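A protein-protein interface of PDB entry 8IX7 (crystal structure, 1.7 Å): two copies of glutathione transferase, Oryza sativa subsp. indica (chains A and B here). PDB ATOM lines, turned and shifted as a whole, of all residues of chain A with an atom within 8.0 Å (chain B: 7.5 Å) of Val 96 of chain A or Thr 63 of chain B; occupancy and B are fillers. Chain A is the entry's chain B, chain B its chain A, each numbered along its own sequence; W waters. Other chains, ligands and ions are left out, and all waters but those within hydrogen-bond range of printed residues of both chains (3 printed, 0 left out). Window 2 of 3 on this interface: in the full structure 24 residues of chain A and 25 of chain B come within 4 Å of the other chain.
Asp 77 of chain B touches Val 95 of chain A. OE1 of Gln 78 of chain B touches CG2 of Val 95 of chain A (3.1 Å). Thr 63 of chain B touches Val 96 of chain A. Gln 78 of chain B touches Val 96 of chain A (OE1 to CG2, 3.9 Å). CG2 of Val 65 of chain B touches CB of Ala 99 of chain A, at 3.9 Å. CD1 of Tyr 74 of chain B touches CB of Ala 99 of chain A, 3.8 Å away.
No position is printed for both chains. Of the 6 pairs that touch across the chains among the printed residues, none has its exchanged pair printed and touching as well.
Asp 93 of chain A touches none of the printed residues of chain B. Printed residues of chain B within 4 Å of Val 95 of chain A: Asp 77 and Gln 78. Val 96 of chain A touches two residues of chain B. Of the printed residues of chain B, Ala 99 of chain A touches Val 65 and Tyr 74. Of chain A, only Val 96 (3.9 Å) comes within 4 Å of Thr 63 of chain B. Of the printed residues of chain A, Val 65 of chain B touches Ala 99. Of the printed residues of chain A, Gln 78 of chain B touches Val 95 and Val 96. The nearest printed residue of chain A that does not touch Gln 78 of chain B is Gly 94 of chain A (6.9 Å).
O of Phe 58 of chain B lies within hydrogen-bond range of N of Val 65 of chain B (3.2 Å). OD1 of Asp 60 of chain B sits at hydrogen-bond distance from N of Thr 63 of chain B (2.8 Å). OD2 of Asp 60 of chain B is in hydrogen-bond range of OH of Tyr 74 of chain B (2.6 Å). The side-chain hydroxyl (OH) of Tyr 74 of chain B sits at hydrogen-bond distance from the side-chain amide oxygen (OE1) of Gln 78 of chain B (3.1 Å).
Printed residues of chain A that touch a printed residue of chain B: Val 95, Val 96 and Ala 99. Along chain A the printed residues that touch a printed residue of chain B span positions 95 to 99. Of the 13 printed residues of chain B, 5 touch a printed residue of chain A. Hydrophobic or aromatic side chains of chain B that line the printed part of chain A: Val 65 and Tyr 74. Among the printed residues, 6 pairs touch across the chains. Among the printed residues, no Asp or Glu carboxylate lies within 4 Å of a Lys or Arg side-chain nitrogen of the other chain.
Water W3 bridges O of Thr 64 of chain B and NZ of Lys 103 of chain A. Water W1 lies within hydrogen-bond range of O of Val 96 of chain A (2.8 Å) and OG1 of Thr 63 of chain B (2.8 Å). Water W2 lies within hydrogen-bond range of the backbone carbonyl oxygen of Thr 64 of chain B and the side-chain amino group of Lys 103 of chain A.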
ATOM      1  N   ARG A  90     -36.458   1.986  15.986  1.00  0.00           N
ATOM      2  CA  ARG A  90     -36.797   0.573  16.087  1.00  0.00           C
ATOM      3  C   ARG A  90     -36.772   0.150  17.548  1.00  0.00           C
ATOM      4  O   ARG A  90     -35.834   0.471  18.276  1.00  0.00           O
ATOM      5  CB  ARG A  90     -35.795  -0.274  15.296  1.00  0.00           C
ATOM      6  CG  ARG A  90     -35.952  -0.174  13.792  1.00  0.00           C
ATOM      7  CD  ARG A  90     -35.114  -1.222  13.079  1.00  0.00           C
ATOM      8  NE  ARG A  90     -35.498  -1.353  11.675  1.00  0.00           N
ATOM      9  CZ  ARG A  90     -36.703  -1.741  11.262  1.00  0.00           C
ATOM     10  NH1 ARG A  90     -37.644  -2.042  12.146  1.00  0.00           N
ATOM     11  NH2 ARG A  90     -36.967  -1.824   9.966  1.00  0.00           N
ATOM     12  N   LYS A  91     -37.806  -0.569  17.972  1.00  0.00           N
ATOM     13  CA  LYS A  91     -37.897  -1.037  19.353  1.00  0.00           C
ATOM     14  C   LYS A  91     -36.598  -1.717  19.775  1.00  0.00           C
ATOM     15  O   LYS A  91     -36.124  -1.540  20.900  1.00  0.00           O
ATOM     16  CB  LYS A  91     -39.050  -2.033  19.501  1.00  0.00           C
ATOM     17  CG  LYS A  91     -40.423  -1.481  19.168  1.00  0.00           C
ATOM     18  CD  LYS A  91     -41.480  -2.568  19.323  1.00  0.00           C
ATOM     19  CE  LYS A  91     -42.872  -2.053  18.995  1.00  0.00           C
ATOM     20  NZ  LYS A  91     -43.897  -3.132  19.113  1.00  0.00           N
ATOM     21  N   GLU A  92     -36.030  -2.492  18.858  1.00  0.00           N
ATOM     22  CA  GLU A  92     -34.800  -3.230  19.108  1.00  0.00           C
ATOM     23  C   GLU A  92     -33.627  -2.346  19.527  1.00  0.00           C
ATOM     24  O   GLU A  92     -32.753  -2.784  20.273  1.00  0.00           O
ATOM     25  CB  GLU A  92     -34.403  -4.025  17.860  1.00  0.00           C
ATOM     26  CG  GLU A  92     -35.489  -4.933  17.294  1.00  0.00           C
ATOM     27  CD  GLU A  92     -36.531  -4.185  16.474  1.00  0.00           C
ATOM     28  OE1 GLU A  92     -37.342  -3.438  17.057  1.00  0.00           O
ATOM     29  OE2 GLU A  92     -36.536  -4.347  15.235  1.00  0.00           O
ATOM     30  N   ASP A  93     -33.608  -1.105  19.047  1.00  0.00           N
ATOM     31  CA  ASP A  93     -32.521  -0.188  19.371  1.00  0.00           C
ATOM     32  C   ASP A  93     -32.731   0.577  20.680  1.00  0.00           C
ATOM     33  O   ASP A  93     -31.848   1.312  21.126  1.00  0.00           O
ATOM     34  CB  ASP A  93     -32.303   0.791  18.210  1.00  0.00           C
ATOM     35  CG  ASP A  93     -31.967   0.081  16.907  1.00  0.00           C
ATOM     36  OD1 ASP A  93     -31.241  -0.937  16.953  1.00  0.00           O
ATOM     37  OD2 ASP A  93     -32.416   0.542  15.836  1.00  0.00           O
ATOM     38  N   GLY A  94     -33.900   0.397  21.284  1.00  0.00           N
ATOM     39  CA  GLY A  94     -34.214   1.041  22.551  1.00  0.00           C
ATOM     40  C   GLY A  94     -33.921   2.525  22.689  1.00  0.00           C
ATOM     41  O   GLY A  94     -34.042   3.288  21.730  1.00  0.00           O
ATOM     42  N   VAL A  95     -33.530   2.926  23.898  1.00  0.00           N
ATOM     43  CA  VAL A  95     -33.232   4.323  24.202  1.00  0.00           C
ATOM     44  C   VAL A  95     -32.032   4.880  23.447  1.00  0.00           C
ATOM     45  O   VAL A  95     -31.989   6.070  23.140  1.00  0.00           O
ATOM     46  CB  VAL A  95     -33.005   4.521  25.714  1.00  0.00           C
ATOM     47  CG1 VAL A  95     -34.289   4.205  26.471  1.00  0.00           C
ATOM     48  CG2 VAL A  95     -31.876   3.623  26.194  1.00  0.00           C
ATOM     49  N   VAL A  96     -31.055   4.028  23.150  1.00  0.00           N
ATOM     50  CA  VAL A  96     -29.883   4.476  22.414  1.00  0.00           C
ATOM     51  C   VAL A  96     -30.321   4.865  21.004  1.00  0.00           C
ATOM     52  O   VAL A  96     -29.825   5.838  20.432  1.00  0.00           O
ATOM     53  CB  VAL A  96     -28.808   3.368  22.349  1.00  0.00           C
ATOM     54  CG1 VAL A  96     -27.672   3.789  21.432  1.00  0.00           C
ATOM     55  CG2 VAL A  96     -28.273   3.093  23.748  1.00  0.00           C
ATOM     56  N   GLY A  97     -31.267   4.105  20.457  1.00  0.00           N
ATOM     57  CA  GLY A  97     -31.772   4.398  19.128  1.00  0.00           C
ATOM     58  C   GLY A  97     -32.561   5.698  19.109  1.00  0.00           C
ATOM     59  O   GLY A  97     -32.482   6.467  18.146  1.00  0.00           O
ATOM     60  N   ARG A  98     -33.325   5.948  20.168  1.00  0.00           N
ATOM     61  CA  ARG A  98     -34.115   7.173  20.249  1.00  0.00           C
ATOM     62  C   ARG A  98     -33.202   8.395  20.330  1.00  0.00           C
ATOM     63  O   ARG A  98     -33.489   9.432  19.734  1.00  0.00           O
ATOM     64  CB  ARG A  98     -35.046   7.134  21.467  1.00  0.00           C
ATOM     65  CG  ARG A  98     -36.205   6.140  21.346  1.00  0.00           C
ATOM     66  CD  ARG A  98     -37.007   6.058  22.646  1.00  0.00           C
ATOM     67  NE  ARG A  98     -37.665   7.318  22.991  1.00  0.00           N
ATOM     68  CZ  ARG A  98     -38.864   7.692  22.552  1.00  0.00           C
ATOM     69  NH1 ARG A  98     -39.556   6.901  21.744  1.00  0.00           N
ATOM     70  NH2 ARG A  98     -39.371   8.860  22.923  1.00  0.00           N
ATOM     71  N   ALA A  99     -32.102   8.271  21.065  1.00  0.00           N
ATOM     72  CA  ALA A  99     -31.158   9.381  21.209  1.00  0.00           C
ATOM     73  C   ALA A  99     -30.545   9.763  19.861  1.00  0.00           C
ATOM     74  O   ALA A  99     -30.295  10.942  19.595  1.00  0.00           O
ATOM     75  CB  ALA A  99     -30.051   9.004  22.203  1.00  0.00           C
ATOM     76  N   ALA A 100     -30.306   8.763  19.015  1.00  0.00           N
ATOM     77  CA  ALA A 100     -29.723   8.990  17.694  1.00  0.00           C
ATOM     78  C   ALA A 100     -30.658   9.832  16.833  1.00  0.00           C
ATOM     79  O   ALA A 100     -30.220  10.477  15.884  1.00  0.00           O
ATOM     80  CB  ALA A 100     -29.438   7.656  17.005  1.00  0.00           C
ATOM     81  N   ILE A 101     -31.946   9.813  17.175  1.00  0.00           N
ATOM     82  CA  ILE A 101     -32.966  10.580  16.464  1.00  0.00           C
ATOM     83  C   ILE A 101     -33.148  11.953  17.123  1.00  0.00           C
ATOM     84  O   ILE A 101     -33.171  12.989  16.451  1.00  0.00           O
ATOM     85  CB  ILE A 101     -34.328   9.830  16.484  1.00  0.00           C
ATOM     86  CG1 ILE A 101     -34.217   8.529  15.683  1.00  0.00           C
ATOM     87  CG2 ILE A 101     -35.435  10.717  15.923  1.00  0.00           C
ATOM     88  CD1 ILE A 101     -35.451   7.647  15.774  1.00  0.00           C
ATOM     89  N   GLU A 102     -33.268  11.950  18.445  1.00  0.00           N
ATOM     90  CA  GLU A 102     -33.457  13.178  19.210  1.00  0.00           C
ATOM     91  C   GLU A 102     -32.404  14.264  18.995  1.00  0.00           C
ATOM     92  O   GLU A 102     -32.735  15.452  18.942  1.00  0.00           O
ATOM     93  CB  GLU A 102     -33.543  12.850  20.704  1.00  0.00           C
ATOM     94  CG  GLU A 102     -34.865  12.234  21.132  1.00  0.00           C
ATOM     95  CD  GLU A 102     -36.001  13.244  21.131  1.00  0.00           C
ATOM     96  OE1 GLU A 102     -35.731  14.447  20.922  1.00  0.00           O
ATOM     97  OE2 GLU A 102     -37.161  12.836  21.351  1.00  0.00           O
ATOM     98  N   LYS A 103     -31.140  13.878  18.868  1.00  0.00           N
ATOM     99  CA  LYS A 103     -30.101  14.879  18.690  1.00  0.00           C
ATOM    100  C   LYS A 103     -30.314  15.696  17.419  1.00  0.00           C
ATOM    101  O   LYS A 103     -30.023  16.888  17.393  1.00  0.00           O
ATOM    102  CB  LYS A 103     -28.707  14.226  18.698  1.00  0.00           C
ATOM    103  CG  LYS A 103     -28.447  13.222  17.584  1.00  0.00           C
ATOM    104  CD  LYS A 103     -27.202  12.398  17.917  1.00  0.00           C
ATOM    105  CE  LYS A 103     -26.883  11.393  16.828  1.00  0.00           C
ATOM    106  NZ  LYS A 103     -25.757  10.494  17.239  1.00  0.00           N
ATOM    107  N   LEU B  49     -17.907  13.812  18.361  1.00  0.00           N
ATOM    108  CA  LEU B  49     -18.877  13.828  19.454  1.00  0.00           C
ATOM    109  C   LEU B  49     -19.928  14.916  19.257  1.00  0.00           C
ATOM    110  O   LEU B  49     -21.092  14.746  19.613  1.00  0.00           O
ATOM    111  CB  LEU B  49     -18.176  14.094  20.787  1.00  0.00           C
ATOM    112  CG  LEU B  49     -17.107  13.128  21.294  1.00  0.00           C
ATOM    113  CD1 LEU B  49     -16.494  13.699  22.570  1.00  0.00           C
ATOM    114  CD2 LEU B  49     -17.720  11.758  21.549  1.00  0.00           C
ATOM    115  N   PHE B  58     -21.455  14.891  25.111  1.00  0.00           N
ATOM    116  CA  PHE B  58     -21.794  13.915  26.146  1.00  0.00           C
ATOM    117  C   PHE B  58     -21.438  12.496  25.725  1.00  0.00           C
ATOM    118  O   PHE B  58     -21.653  12.104  24.580  1.00  0.00           O
ATOM    119  CB  PHE B  58     -23.296  13.990  26.447  1.00  0.00           C
ATOM    120  CG  PHE B  58     -23.783  12.942  27.411  1.00  0.00           C
ATOM    121  CD1 PHE B  58     -23.696  13.141  28.786  1.00  0.00           C
ATOM    122  CD2 PHE B  58     -24.336  11.753  26.942  1.00  0.00           C
ATOM    123  CE1 PHE B  58     -24.154  12.173  29.677  1.00  0.00           C
ATOM    124  CE2 PHE B  58     -24.795  10.779  27.824  1.00  0.00           C
ATOM    125  CZ  PHE B  58     -24.705  10.990  29.194  1.00  0.00           C
ATOM    126  N   LYS B  59     -20.900  11.721  26.660  1.00  0.00           N
ATOM    127  CA  LYS B  59     -20.541  10.344  26.366  1.00  0.00           C
ATOM    128  C   LYS B  59     -20.635   9.465  27.601  1.00  0.00           C
ATOM    129  O   LYS B  59     -20.245   9.875  28.691  1.00  0.00           O
ATOM    130  CB  LYS B  59     -19.114  10.272  25.811  1.00  0.00           C
ATOM    131  CG  LYS B  59     -18.585   8.852  25.647  1.00  0.00           C
ATOM    132  CD  LYS B  59     -17.131   8.840  25.202  1.00  0.00           C
ATOM    133  CE  LYS B  59     -16.603   7.416  25.091  1.00  0.00           C
ATOM    134  NZ  LYS B  59     -15.179   7.380  24.657  1.00  0.00           N
ATOM    135  N   ASP B  60     -21.185   8.265  27.425  1.00  0.00           N
ATOM    136  CA  ASP B  60     -21.270   7.294  28.513  1.00  0.00           C
ATOM    137  C   ASP B  60     -20.828   5.947  27.939  1.00  0.00           C
ATOM    138  O   ASP B  60     -20.357   5.892  26.804  1.00  0.00           O
ATOM    139  CB  ASP B  60     -22.685   7.237  29.124  1.00  0.00           C
ATOM    140  CG  ASP B  60     -23.721   6.614  28.207  1.00  0.00           C
ATOM    141  OD1 ASP B  60     -23.384   6.200  27.078  1.00  0.00           O
ATOM    142  OD2 ASP B  60     -24.893   6.540  28.640  1.00  0.00           O
ATOM    143  N   SER B  61     -20.959   4.867  28.704  1.00  0.00           N
ATOM    144  CA  SER B  61     -20.516   3.558  28.223  1.00  0.00           C
ATOM    145  C   SER B  61     -21.359   2.952  27.105  1.00  0.00           C
ATOM    146  O   SER B  61     -20.977   1.935  26.523  1.00  0.00           O
ATOM    147  CB  SER B  61     -20.448   2.564  29.388  1.00  0.00           C
ATOM    148  OG  SER B  61     -21.734   2.343  29.936  1.00  0.00           O
ATOM    149  N   LEU B  62     -22.492   3.569  26.789  1.00  0.00           N
ATOM    150  CA  LEU B  62     -23.357   3.027  25.748  1.00  0.00           C
ATOM    151  C   LEU B  62     -23.364   3.800  24.436  1.00  0.00           C
ATOM    152  O   LEU B  62     -23.487   3.207  23.362  1.00  0.00           O
ATOM    153  CB  LEU B  62     -24.796   2.922  26.265  1.00  0.00           C
ATOM    154  CG  LEU B  62     -25.053   2.045  27.494  1.00  0.00           C
ATOM    155  CD1 LEU B  62     -26.533   2.090  27.843  1.00  0.00           C
ATOM    156  CD2 LEU B  62     -24.621   0.616  27.218  1.00  0.00           C
ATOM    157  N   THR B  63     -23.226   5.119  24.510  1.00  0.00           N
ATOM    158  CA  THR B  63     -23.277   5.921  23.295  1.00  0.00           C
ATOM    159  C   THR B  63     -22.814   7.353  23.538  1.00  0.00           C
ATOM    160  O   THR B  63     -22.296   7.679  24.605  1.00  0.00           O
ATOM    161  CB  THR B  63     -24.734   5.942  22.756  1.00  0.00           C
ATOM    162  OG1 THR B  63     -24.781   6.589  21.478  1.00  0.00           O
ATOM    163  CG2 THR B  63     -25.646   6.676  23.734  1.00  0.00           C
ATOM    164  N   THR B  64     -22.990   8.198  22.527  1.00  0.00           N
ATOM    165  CA  THR B  64     -22.639   9.607  22.626  1.00  0.00           C
ATOM    166  C   THR B  64     -23.848  10.359  22.090  1.00  0.00           C
ATOM    167  O   THR B  64     -24.533   9.874  21.190  1.00  0.00           O
ATOM    168  CB  THR B  64     -21.396   9.976  21.775  1.00  0.00           C
ATOM    169  OG1 THR B  64     -21.696   9.826  20.382  1.00  0.00           O
ATOM    170  CG2 THR B  64     -20.221   9.076  22.131  1.00  0.00           C
ATOM    171  N   VAL B  65     -24.124  11.524  22.660  1.00  0.00           N
ATOM    172  CA  VAL B  65     -25.263  12.328  22.226  1.00  0.00           C
ATOM    173  C   VAL B  65     -24.884  13.804  22.274  1.00  0.00           C
ATOM    174  O   VAL B  65     -24.057  14.203  23.095  1.00  0.00           O
ATOM    175  CB  VAL B  65     -26.489  12.130  23.159  1.00  0.00           C
ATOM    176  CG1 VAL B  65     -27.731  12.734  22.518  1.00  0.00           C
ATOM    177  CG2 VAL B  65     -26.703  10.652  23.464  1.00  0.00           C
ATOM    178  N   TYR B  74     -32.221  11.677  26.944  1.00  0.00           N
ATOM    179  CA  TYR B  74     -31.528  10.391  26.955  1.00  0.00           C
ATOM    180  C   TYR B  74     -31.255   9.951  28.390  1.00  0.00           C
ATOM    181  O   TYR B  74     -31.525   8.807  28.769  1.00  0.00           O
ATOM    182  CB  TYR B  74     -30.198  10.498  26.202  1.00  0.00           C
ATOM    183  CG  TYR B  74     -29.302   9.298  26.405  1.00  0.00           C
ATOM    184  CD1 TYR B  74     -29.595   8.072  25.807  1.00  0.00           C
ATOM    185  CD2 TYR B  74     -28.186   9.376  27.237  1.00  0.00           C
ATOM    186  CE1 TYR B  74     -28.796   6.948  26.039  1.00  0.00           C
ATOM    187  CE2 TYR B  74     -27.382   8.256  27.478  1.00  0.00           C
ATOM    188  CZ  TYR B  74     -27.696   7.047  26.876  1.00  0.00           C
ATOM    189  OH  TYR B  74     -26.922   5.934  27.124  1.00  0.00           O
ATOM    190  N   ASP B  77     -34.294   8.714  30.204  1.00  0.00           N
ATOM    191  CA  ASP B  77     -34.802   7.422  29.750  1.00  0.00           C
ATOM    192  C   ASP B  77     -33.851   6.273  30.070  1.00  0.00           C
ATOM    193  O   ASP B  77     -34.283   5.199  30.492  1.00  0.00           O
ATOM    194  CB  ASP B  77     -35.075   7.446  28.244  1.00  0.00           C
ATOM    195  CG  ASP B  77     -36.263   8.313  27.883  1.00  0.00           C
ATOM    196  OD1 ASP B  77     -37.303   8.217  28.569  1.00  0.00           O
ATOM    197  OD2 ASP B  77     -36.166   9.084  26.905  1.00  0.00           O
ATOM    198  N   GLN B  78     -32.557   6.503  29.874  1.00  0.00           N
ATOM    199  CA  GLN B  78     -31.540   5.486  30.130  1.00  0.00           C
ATOM    200  C   GLN B  78     -31.338   5.175  31.614  1.00  0.00           C
ATOM    201  O   GLN B  78     -31.090   4.024  31.985  1.00  0.00           O
ATOM    202  CB  GLN B  78     -30.202   5.923  29.532  1.00  0.00           C
ATOM    203  CG  GLN B  78     -29.106   4.880  29.652  1.00  0.00           C
ATOM    204  CD  GLN B  78     -29.338   3.701  28.733  1.00  0.00           C
ATOM    205  OE1 GLN B  78     -29.104   3.786  27.525  1.00  0.00           O
ATOM    206  NE2 GLN B  78     -29.811   2.598  29.292  1.00  0.00           N
ATOM    207  N   TYR B  79     -31.436   6.198  32.457  1.00  0.00           N
ATOM    208  CA  TYR B  79     -31.238   6.033  33.898  1.00  0.00           C
ATOM    209  C   TYR B  79     -32.532   6.328  34.656  1.00  0.00           C
ATOM    210  O   TYR B  79     -32.516   6.891  35.753  1.00  0.00           O
ATOM    211  CB  TYR B  79     -30.128   6.983  34.363  1.00  0.00           C
ATOM    212  CG  TYR B  79     -28.819   6.793  33.624  1.00  0.00           C
ATOM    213  CD1 TYR B  79     -27.886   5.847  34.048  1.00  0.00           C
ATOM    214  CD2 TYR B  79     -28.528   7.537  32.482  1.00  0.00           C
ATOM    215  CE1 TYR B  79     -26.693   5.646  33.352  1.00  0.00           C
ATOM    216  CE2 TYR B  79     -27.339   7.343  31.778  1.00  0.00           C
ATOM    217  CZ  TYR B  79     -26.428   6.397  32.218  1.00  0.00           C
ATOM    218  OH  TYR B  79     -25.261   6.195  31.519  1.00  0.00           O
HETATM  219  O   HOH W   1     -27.232   6.845  20.146  1.00  0.00           O
HETATM  220  O   HOH W   2     -23.786   8.499  18.620  1.00  0.00           O
HETATM  221  O   HOH W   3     -26.848   9.557  19.785  1.00  0.00           O
